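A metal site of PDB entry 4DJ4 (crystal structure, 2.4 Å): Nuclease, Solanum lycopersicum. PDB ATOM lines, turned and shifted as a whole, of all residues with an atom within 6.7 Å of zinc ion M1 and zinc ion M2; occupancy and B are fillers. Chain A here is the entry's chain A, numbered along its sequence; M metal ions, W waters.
The nearest printed residue that does not touch zinc ion M2 is Ser 2 (4.2 Å).
The nearest printed residue that does not touch zinc ion M1 is His 132 (4.1 Å).
N of Trp 1 sits close to OD1 of Asp 160, at 3.1 Å. The indole nitrogen (NE1) of Trp 1 lies within hydrogen-bond range of the backbone carbonyl oxygen (O) of Gly 125 (3.0 Å). A ring nitrogen (ND1) of His 132 lies within hydrogen-bond range of the backbone carbonyl oxygen (O) of His 60, 2.5 Å away. The guanidinium group (NE) of Arg 48 lies within hydrogen-bond range of the backbone carbonyl oxygen (O) of Asp 45 (3.3 Å).
Zinc ion M2 is bound by a ring nitrogen (NE2) of His 6, the backbone nitrogen (N) of Trp 1, the side-chain carboxylate (OD1) of Asp 126, water W3 and the backbone carbonyl oxygen (O) of Trp 1. Zinc ion M2 has five donor atoms within binding distance.
Water W3 binds zinc ion M1, 1.9 Å away. A ring nitrogen (NE2) of His 122 is bound to zinc ion M1, at 2.1 Å. OD2 of Asp 126 is bound to zinc ion M1 (2.2 Å). Zinc ion M1 is bound by ND1 of His 60, at 2.2 Å. Water W1 is bound to zinc ion M1, at 2.5 Å. OD1 of Asp 45 binds zinc ion M1, at 2.5 Å.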
ATOM      1  N   TRP A   1      31.523 -17.586 -16.741  1.00  0.00           N
ATOM      2  CA  TRP A   1      32.018 -17.695 -18.147  1.00  0.00           C
ATOM      3  C   TRP A   1      31.289 -16.700 -18.995  1.00  0.00           C
ATOM      4  O   TRP A   1      30.118 -16.341 -18.713  1.00  0.00           O
ATOM      5  CB  TRP A   1      31.754 -19.078 -18.764  1.00  0.00           C
ATOM      6  CG  TRP A   1      32.368 -20.263 -18.083  1.00  0.00           C
ATOM      7  CD1 TRP A   1      31.716 -21.239 -17.348  1.00  0.00           C
ATOM      8  CD2 TRP A   1      33.777 -20.694 -18.090  1.00  0.00           C
ATOM      9  NE1 TRP A   1      32.591 -22.185 -16.891  1.00  0.00           N
ATOM     10  CE2 TRP A   1      33.837 -21.916 -17.299  1.00  0.00           C
ATOM     11  CE3 TRP A   1      34.951 -20.200 -18.643  1.00  0.00           C
ATOM     12  CZ2 TRP A   1      35.030 -22.602 -17.102  1.00  0.00           C
ATOM     13  CZ3 TRP A   1      36.139 -20.889 -18.433  1.00  0.00           C
ATOM     14  CH2 TRP A   1      36.187 -22.063 -17.679  1.00  0.00           C
ATOM     15  N   SER A   2      31.946 -16.297 -20.094  1.00  0.00           N
ATOM     16  CA  SER A   2      31.231 -15.650 -21.183  1.00  0.00           C
ATOM     17  C   SER A   2      30.412 -16.741 -21.935  1.00  0.00           C
ATOM     18  O   SER A   2      30.386 -17.885 -21.524  1.00  0.00           O
ATOM     19  CB  SER A   2      32.196 -14.928 -22.120  1.00  0.00           C
ATOM     20  OG  SER A   2      32.937 -13.907 -21.437  1.00  0.00           O
ATOM     21  N   LYS A   3      29.752 -16.355 -23.018  1.00  0.00           N
ATOM     22  CA  LYS A   3      28.821 -17.175 -23.755  1.00  0.00           C
ATOM     23  C   LYS A   3      29.320 -18.620 -24.002  1.00  0.00           C
ATOM     24  O   LYS A   3      28.642 -19.589 -23.676  1.00  0.00           O
ATOM     25  CB  LYS A   3      28.545 -16.463 -25.080  1.00  0.00           C
ATOM     26  CG  LYS A   3      27.358 -16.929 -25.900  1.00  0.00           C
ATOM     27  CD  LYS A   3      27.548 -16.550 -27.372  1.00  0.00           C
ATOM     28  CE  LYS A   3      27.807 -15.049 -27.584  1.00  0.00           C
ATOM     29  NZ  LYS A   3      28.769 -14.776 -28.709  1.00  0.00           N
ATOM     30  N   GLY A   5      31.721 -20.604 -22.727  1.00  0.00           N
ATOM     31  CA  GLY A   5      31.912 -21.524 -21.625  1.00  0.00           C
ATOM     32  C   GLY A   5      30.590 -22.097 -21.168  1.00  0.00           C
ATOM     33  O   GLY A   5      30.500 -23.283 -20.853  1.00  0.00           O
ATOM     34  N   HIS A   6      29.556 -21.246 -21.143  1.00  0.00           N
ATOM     35  CA  HIS A   6      28.228 -21.715 -20.793  1.00  0.00           C
ATOM     36  C   HIS A   6      27.639 -22.652 -21.817  1.00  0.00           C
ATOM     37  O   HIS A   6      27.105 -23.702 -21.446  1.00  0.00           O
ATOM     38  CB  HIS A   6      27.288 -20.566 -20.455  1.00  0.00           C
ATOM     39  CG  HIS A   6      27.651 -19.887 -19.184  1.00  0.00           C
ATOM     40  ND1 HIS A   6      27.544 -20.497 -17.990  1.00  0.00           N
ATOM     41  CD2 HIS A   6      28.218 -18.624 -18.931  1.00  0.00           C
ATOM     42  CE1 HIS A   6      28.009 -19.670 -17.030  1.00  0.00           C
ATOM     43  NE2 HIS A   6      28.383 -18.516 -17.609  1.00  0.00           N
ATOM     44  N   VAL A  42      23.106 -18.694 -21.061  1.00  0.00           N
ATOM     45  CA  VAL A  42      23.715 -17.406 -20.756  1.00  0.00           C
ATOM     46  C   VAL A  42      22.647 -16.397 -20.277  1.00  0.00           C
ATOM     47  O   VAL A  42      22.983 -15.265 -19.854  1.00  0.00           O
ATOM     48  CB  VAL A  42      24.554 -16.922 -21.986  1.00  0.00           C
ATOM     49  CG1 VAL A  42      23.688 -16.364 -23.097  1.00  0.00           C
ATOM     50  CG2 VAL A  42      25.628 -15.920 -21.553  1.00  0.00           C
ATOM     51  N   PRO A  44      20.873 -16.006 -17.597  1.00  0.00           N
ATOM     52  CA  PRO A  44      21.029 -15.251 -16.333  1.00  0.00           C
ATOM     53  C   PRO A  44      21.993 -14.051 -16.366  1.00  0.00           C
ATOM     54  O   PRO A  44      21.860 -13.152 -15.552  1.00  0.00           O
ATOM     55  CB  PRO A  44      21.545 -16.322 -15.348  1.00  0.00           C
ATOM     56  CG  PRO A  44      21.018 -17.605 -15.900  1.00  0.00           C
ATOM     57  CD  PRO A  44      21.074 -17.458 -17.402  1.00  0.00           C
ATOM     58  N   ASP A  45      22.970 -14.047 -17.285  1.00  0.00           N
ATOM     59  CA  ASP A  45      23.912 -12.919 -17.376  1.00  0.00           C
ATOM     60  C   ASP A  45      23.238 -11.652 -17.941  1.00  0.00           C
ATOM     61  O   ASP A  45      23.702 -10.542 -17.688  1.00  0.00           O
ATOM     62  CB  ASP A  45      25.134 -13.256 -18.252  1.00  0.00           C
ATOM     63  CG  ASP A  45      26.257 -13.927 -17.466  1.00  0.00           C
ATOM     64  OD1 ASP A  45      26.219 -13.963 -16.222  1.00  0.00           O
ATOM     65  OD2 ASP A  45      27.190 -14.439 -18.111  1.00  0.00           O
ATOM     66  N   ARG A  48      20.269 -10.524 -14.951  1.00  0.00           N
ATOM     67  CA  ARG A  48      20.735 -10.059 -13.622  1.00  0.00           C
ATOM     68  C   ARG A  48      20.652  -8.505 -13.462  1.00  0.00           C
ATOM     69  O   ARG A  48      20.621  -8.000 -12.337  1.00  0.00           O
ATOM     70  CB  ARG A  48      22.159 -10.553 -13.324  1.00  0.00           C
ATOM     71  CG  ARG A  48      23.247  -9.920 -14.172  1.00  0.00           C
ATOM     72  CD  ARG A  48      24.618 -10.498 -13.845  1.00  0.00           C
ATOM     73  NE  ARG A  48      25.544 -10.317 -14.968  1.00  0.00           N
ATOM     74  CZ  ARG A  48      26.516  -9.411 -15.052  1.00  0.00           C
ATOM     75  NH1 ARG A  48      26.736  -8.530 -14.057  1.00  0.00           N
ATOM     76  NH2 ARG A  48      27.274  -9.369 -16.148  1.00  0.00           N
ATOM     77  N   LEU A  59      24.849 -14.023  -7.043  1.00  0.00           N
ATOM     78  CA  LEU A  59      24.821 -15.485  -7.203  1.00  0.00           C
ATOM     79  C   LEU A  59      25.782 -16.033  -8.288  1.00  0.00           C
ATOM     80  O   LEU A  59      25.837 -17.250  -8.516  1.00  0.00           O
ATOM     81  CB  LEU A  59      23.387 -15.953  -7.470  1.00  0.00           C
ATOM     82  CG  LEU A  59      22.329 -15.578  -6.402  1.00  0.00           C
ATOM     83  CD1 LEU A  59      21.054 -16.363  -6.672  1.00  0.00           C
ATOM     84  CD2 LEU A  59      22.768 -15.797  -4.944  1.00  0.00           C
ATOM     85  N   HIS A  60      26.528 -15.139  -8.942  1.00  0.00           N
ATOM     86  CA  HIS A  60      27.394 -15.521 -10.071  1.00  0.00           C
ATOM     87  C   HIS A  60      28.793 -15.847  -9.622  1.00  0.00           C
ATOM     88  O   HIS A  60      29.569 -16.441 -10.375  1.00  0.00           O
ATOM     89  CB  HIS A  60      27.407 -14.402 -11.134  1.00  0.00           C
ATOM     90  CG  HIS A  60      26.131 -14.320 -11.943  1.00  0.00           C
ATOM     91  ND1 HIS A  60      26.035 -14.808 -13.209  1.00  0.00           N
ATOM     92  CD2 HIS A  60      24.877 -13.831 -11.618  1.00  0.00           C
ATOM     93  CE1 HIS A  60      24.775 -14.623 -13.668  1.00  0.00           C
ATOM     94  NE2 HIS A  60      24.056 -14.040 -12.697  1.00  0.00           N
ATOM     95  N   PHE A  61      29.131 -15.504  -8.378  1.00  0.00           N
ATOM     96  CA  PHE A  61      30.517 -15.561  -7.948  1.00  0.00           C
ATOM     97  C   PHE A  61      30.636 -15.733  -6.453  1.00  0.00           C
ATOM     98  O   PHE A  61      29.646 -15.678  -5.723  1.00  0.00           O
ATOM     99  CB  PHE A  61      31.260 -14.281  -8.379  1.00  0.00           C
ATOM    100  CG  PHE A  61      30.727 -13.026  -7.738  1.00  0.00           C
ATOM    101  CD1 PHE A  61      31.007 -12.718  -6.400  1.00  0.00           C
ATOM    102  CD2 PHE A  61      29.924 -12.146  -8.465  1.00  0.00           C
ATOM    103  CE1 PHE A  61      30.498 -11.562  -5.792  1.00  0.00           C
ATOM    104  CE2 PHE A  61      29.411 -10.984  -7.864  1.00  0.00           C
ATOM    105  CZ  PHE A  61      29.707 -10.695  -6.533  1.00  0.00           C
ATOM    106  N   HIS A 122      23.497 -22.277 -15.430  1.00  0.00           N
ATOM    107  CA  HIS A 122      24.436 -21.182 -15.530  1.00  0.00           C
ATOM    108  C   HIS A 122      25.414 -21.178 -14.372  1.00  0.00           C
ATOM    109  O   HIS A 122      26.642 -21.089 -14.586  1.00  0.00           O
ATOM    110  CB  HIS A 122      23.683 -19.838 -15.601  1.00  0.00           C
ATOM    111  CG  HIS A 122      24.599 -18.661 -15.843  1.00  0.00           C
ATOM    112  ND1 HIS A 122      24.896 -18.228 -17.084  1.00  0.00           N
ATOM    113  CD2 HIS A 122      25.299 -17.838 -14.955  1.00  0.00           C
ATOM    114  CE1 HIS A 122      25.742 -17.181 -16.990  1.00  0.00           C
ATOM    115  NE2 HIS A 122      25.980 -16.945 -15.686  1.00  0.00           N
ATOM    116  N   PHE A 123      24.879 -21.281 -13.159  1.00  0.00           N
ATOM    117  CA  PHE A 123      25.675 -21.152 -11.956  1.00  0.00           C
ATOM    118  C   PHE A 123      26.568 -22.368 -11.748  1.00  0.00           C
ATOM    119  O   PHE A 123      27.610 -22.242 -11.115  1.00  0.00           O
ATOM    120  CB  PHE A 123      24.805 -20.903 -10.723  1.00  0.00           C
ATOM    121  CG  PHE A 123      24.093 -19.598 -10.735  1.00  0.00           C
ATOM    122  CD1 PHE A 123      24.747 -18.438 -11.120  1.00  0.00           C
ATOM    123  CD2 PHE A 123      22.769 -19.517 -10.310  1.00  0.00           C
ATOM    124  CE1 PHE A 123      24.098 -17.206 -11.137  1.00  0.00           C
ATOM    125  CE2 PHE A 123      22.108 -18.296 -10.341  1.00  0.00           C
ATOM    126  CZ  PHE A 123      22.775 -17.134 -10.744  1.00  0.00           C
ATOM    127  N   GLY A 125      28.190 -23.631 -14.222  1.00  0.00           N
ATOM    128  CA  GLY A 125      29.326 -23.179 -15.015  1.00  0.00           C
ATOM    129  C   GLY A 125      30.173 -22.150 -14.269  1.00  0.00           C
ATOM    130  O   GLY A 125      31.397 -22.293 -14.175  1.00  0.00           O
ATOM    131  N   ASP A 126      29.518 -21.135 -13.711  1.00  0.00           N
ATOM    132  CA  ASP A 126      30.265 -20.051 -13.064  1.00  0.00           C
ATOM    133  C   ASP A 126      31.129 -20.470 -11.901  1.00  0.00           C
ATOM    134  O   ASP A 126      32.234 -19.991 -11.779  1.00  0.00           O
ATOM    135  CB  ASP A 126      29.336 -18.932 -12.568  1.00  0.00           C
ATOM    136  CG  ASP A 126      28.956 -17.969 -13.656  1.00  0.00           C
ATOM    137  OD1 ASP A 126      29.524 -18.038 -14.786  1.00  0.00           O
ATOM    138  OD2 ASP A 126      28.064 -17.130 -13.359  1.00  0.00           O
ATOM    139  N   GLN A 129      34.405 -21.758 -13.047  1.00  0.00           N
ATOM    140  CA  GLN A 129      35.335 -20.752 -13.584  1.00  0.00           C
ATOM    141  C   GLN A 129      36.140 -20.227 -12.381  1.00  0.00           C
ATOM    142  O   GLN A 129      35.596 -19.497 -11.542  1.00  0.00           O
ATOM    143  CB  GLN A 129      34.541 -19.615 -14.256  1.00  0.00           C
ATOM    144  CG  GLN A 129      35.238 -18.893 -15.388  1.00  0.00           C
ATOM    145  CD  GLN A 129      36.393 -18.010 -14.935  1.00  0.00           C
ATOM    146  OE1 GLN A 129      37.366 -18.505 -14.333  1.00  0.00           O
ATOM    147  NE2 GLN A 129      36.322 -16.696 -15.266  1.00  0.00           N
ATOM    148  N   HIS A 132      35.785 -16.785 -10.937  1.00  0.00           N
ATOM    149  CA  HIS A 132      34.502 -16.487 -10.302  1.00  0.00           C
ATOM    150  C   HIS A 132      34.527 -16.754  -8.833  1.00  0.00           C
ATOM    151  O   HIS A 132      33.549 -16.513  -8.143  1.00  0.00           O
ATOM    152  CB  HIS A 132      33.335 -17.260 -10.947  1.00  0.00           C
ATOM    153  CG  HIS A 132      32.663 -16.504 -12.054  1.00  0.00           C
ATOM    154  ND1 HIS A 132      31.378 -16.132 -12.002  1.00  0.00           N
ATOM    155  CD2 HIS A 132      33.156 -16.028 -13.261  1.00  0.00           C
ATOM    156  CE1 HIS A 132      31.077 -15.437 -13.102  1.00  0.00           C
ATOM    157  NE2 HIS A 132      32.168 -15.380 -13.875  1.00  0.00           N
ATOM    158  N   ASP A 160      37.135 -15.987 -18.408  1.00  0.00           N
ATOM    159  CA  ASP A 160      35.777 -16.054 -18.930  1.00  0.00           C
ATOM    160  C   ASP A 160      35.720 -16.321 -20.448  1.00  0.00           C
ATOM    161  O   ASP A 160      34.735 -16.889 -20.907  1.00  0.00           O
ATOM    162  CB  ASP A 160      35.014 -14.721 -18.697  1.00  0.00           C
ATOM    163  CG  ASP A 160      34.208 -14.671 -17.417  1.00  0.00           C
ATOM    164  OD1 ASP A 160      34.044 -15.702 -16.724  1.00  0.00           O
ATOM    165  OD2 ASP A 160      33.715 -13.579 -17.091  1.00  0.00           O
HETATM  166 ZN    ZN M   1      27.346 -15.624 -14.804  1.00  0.00          ZN
HETATM  167 ZN    ZN M   2      29.585 -17.242 -16.712  1.00  0.00          ZN
HETATM  168 ZN    ZN M   3      32.766 -13.823 -15.351  1.00  0.00          ZN
HETATM  169  O   HOH W   1      28.421 -13.489 -14.245  1.00  0.00           O
HETATM  170  O   HOH W   2      30.988 -14.349 -16.712  1.00  0.00           O
HETATM  171  O   HOH W   3      28.781 -15.411 -16.102  1.00  0.00           O
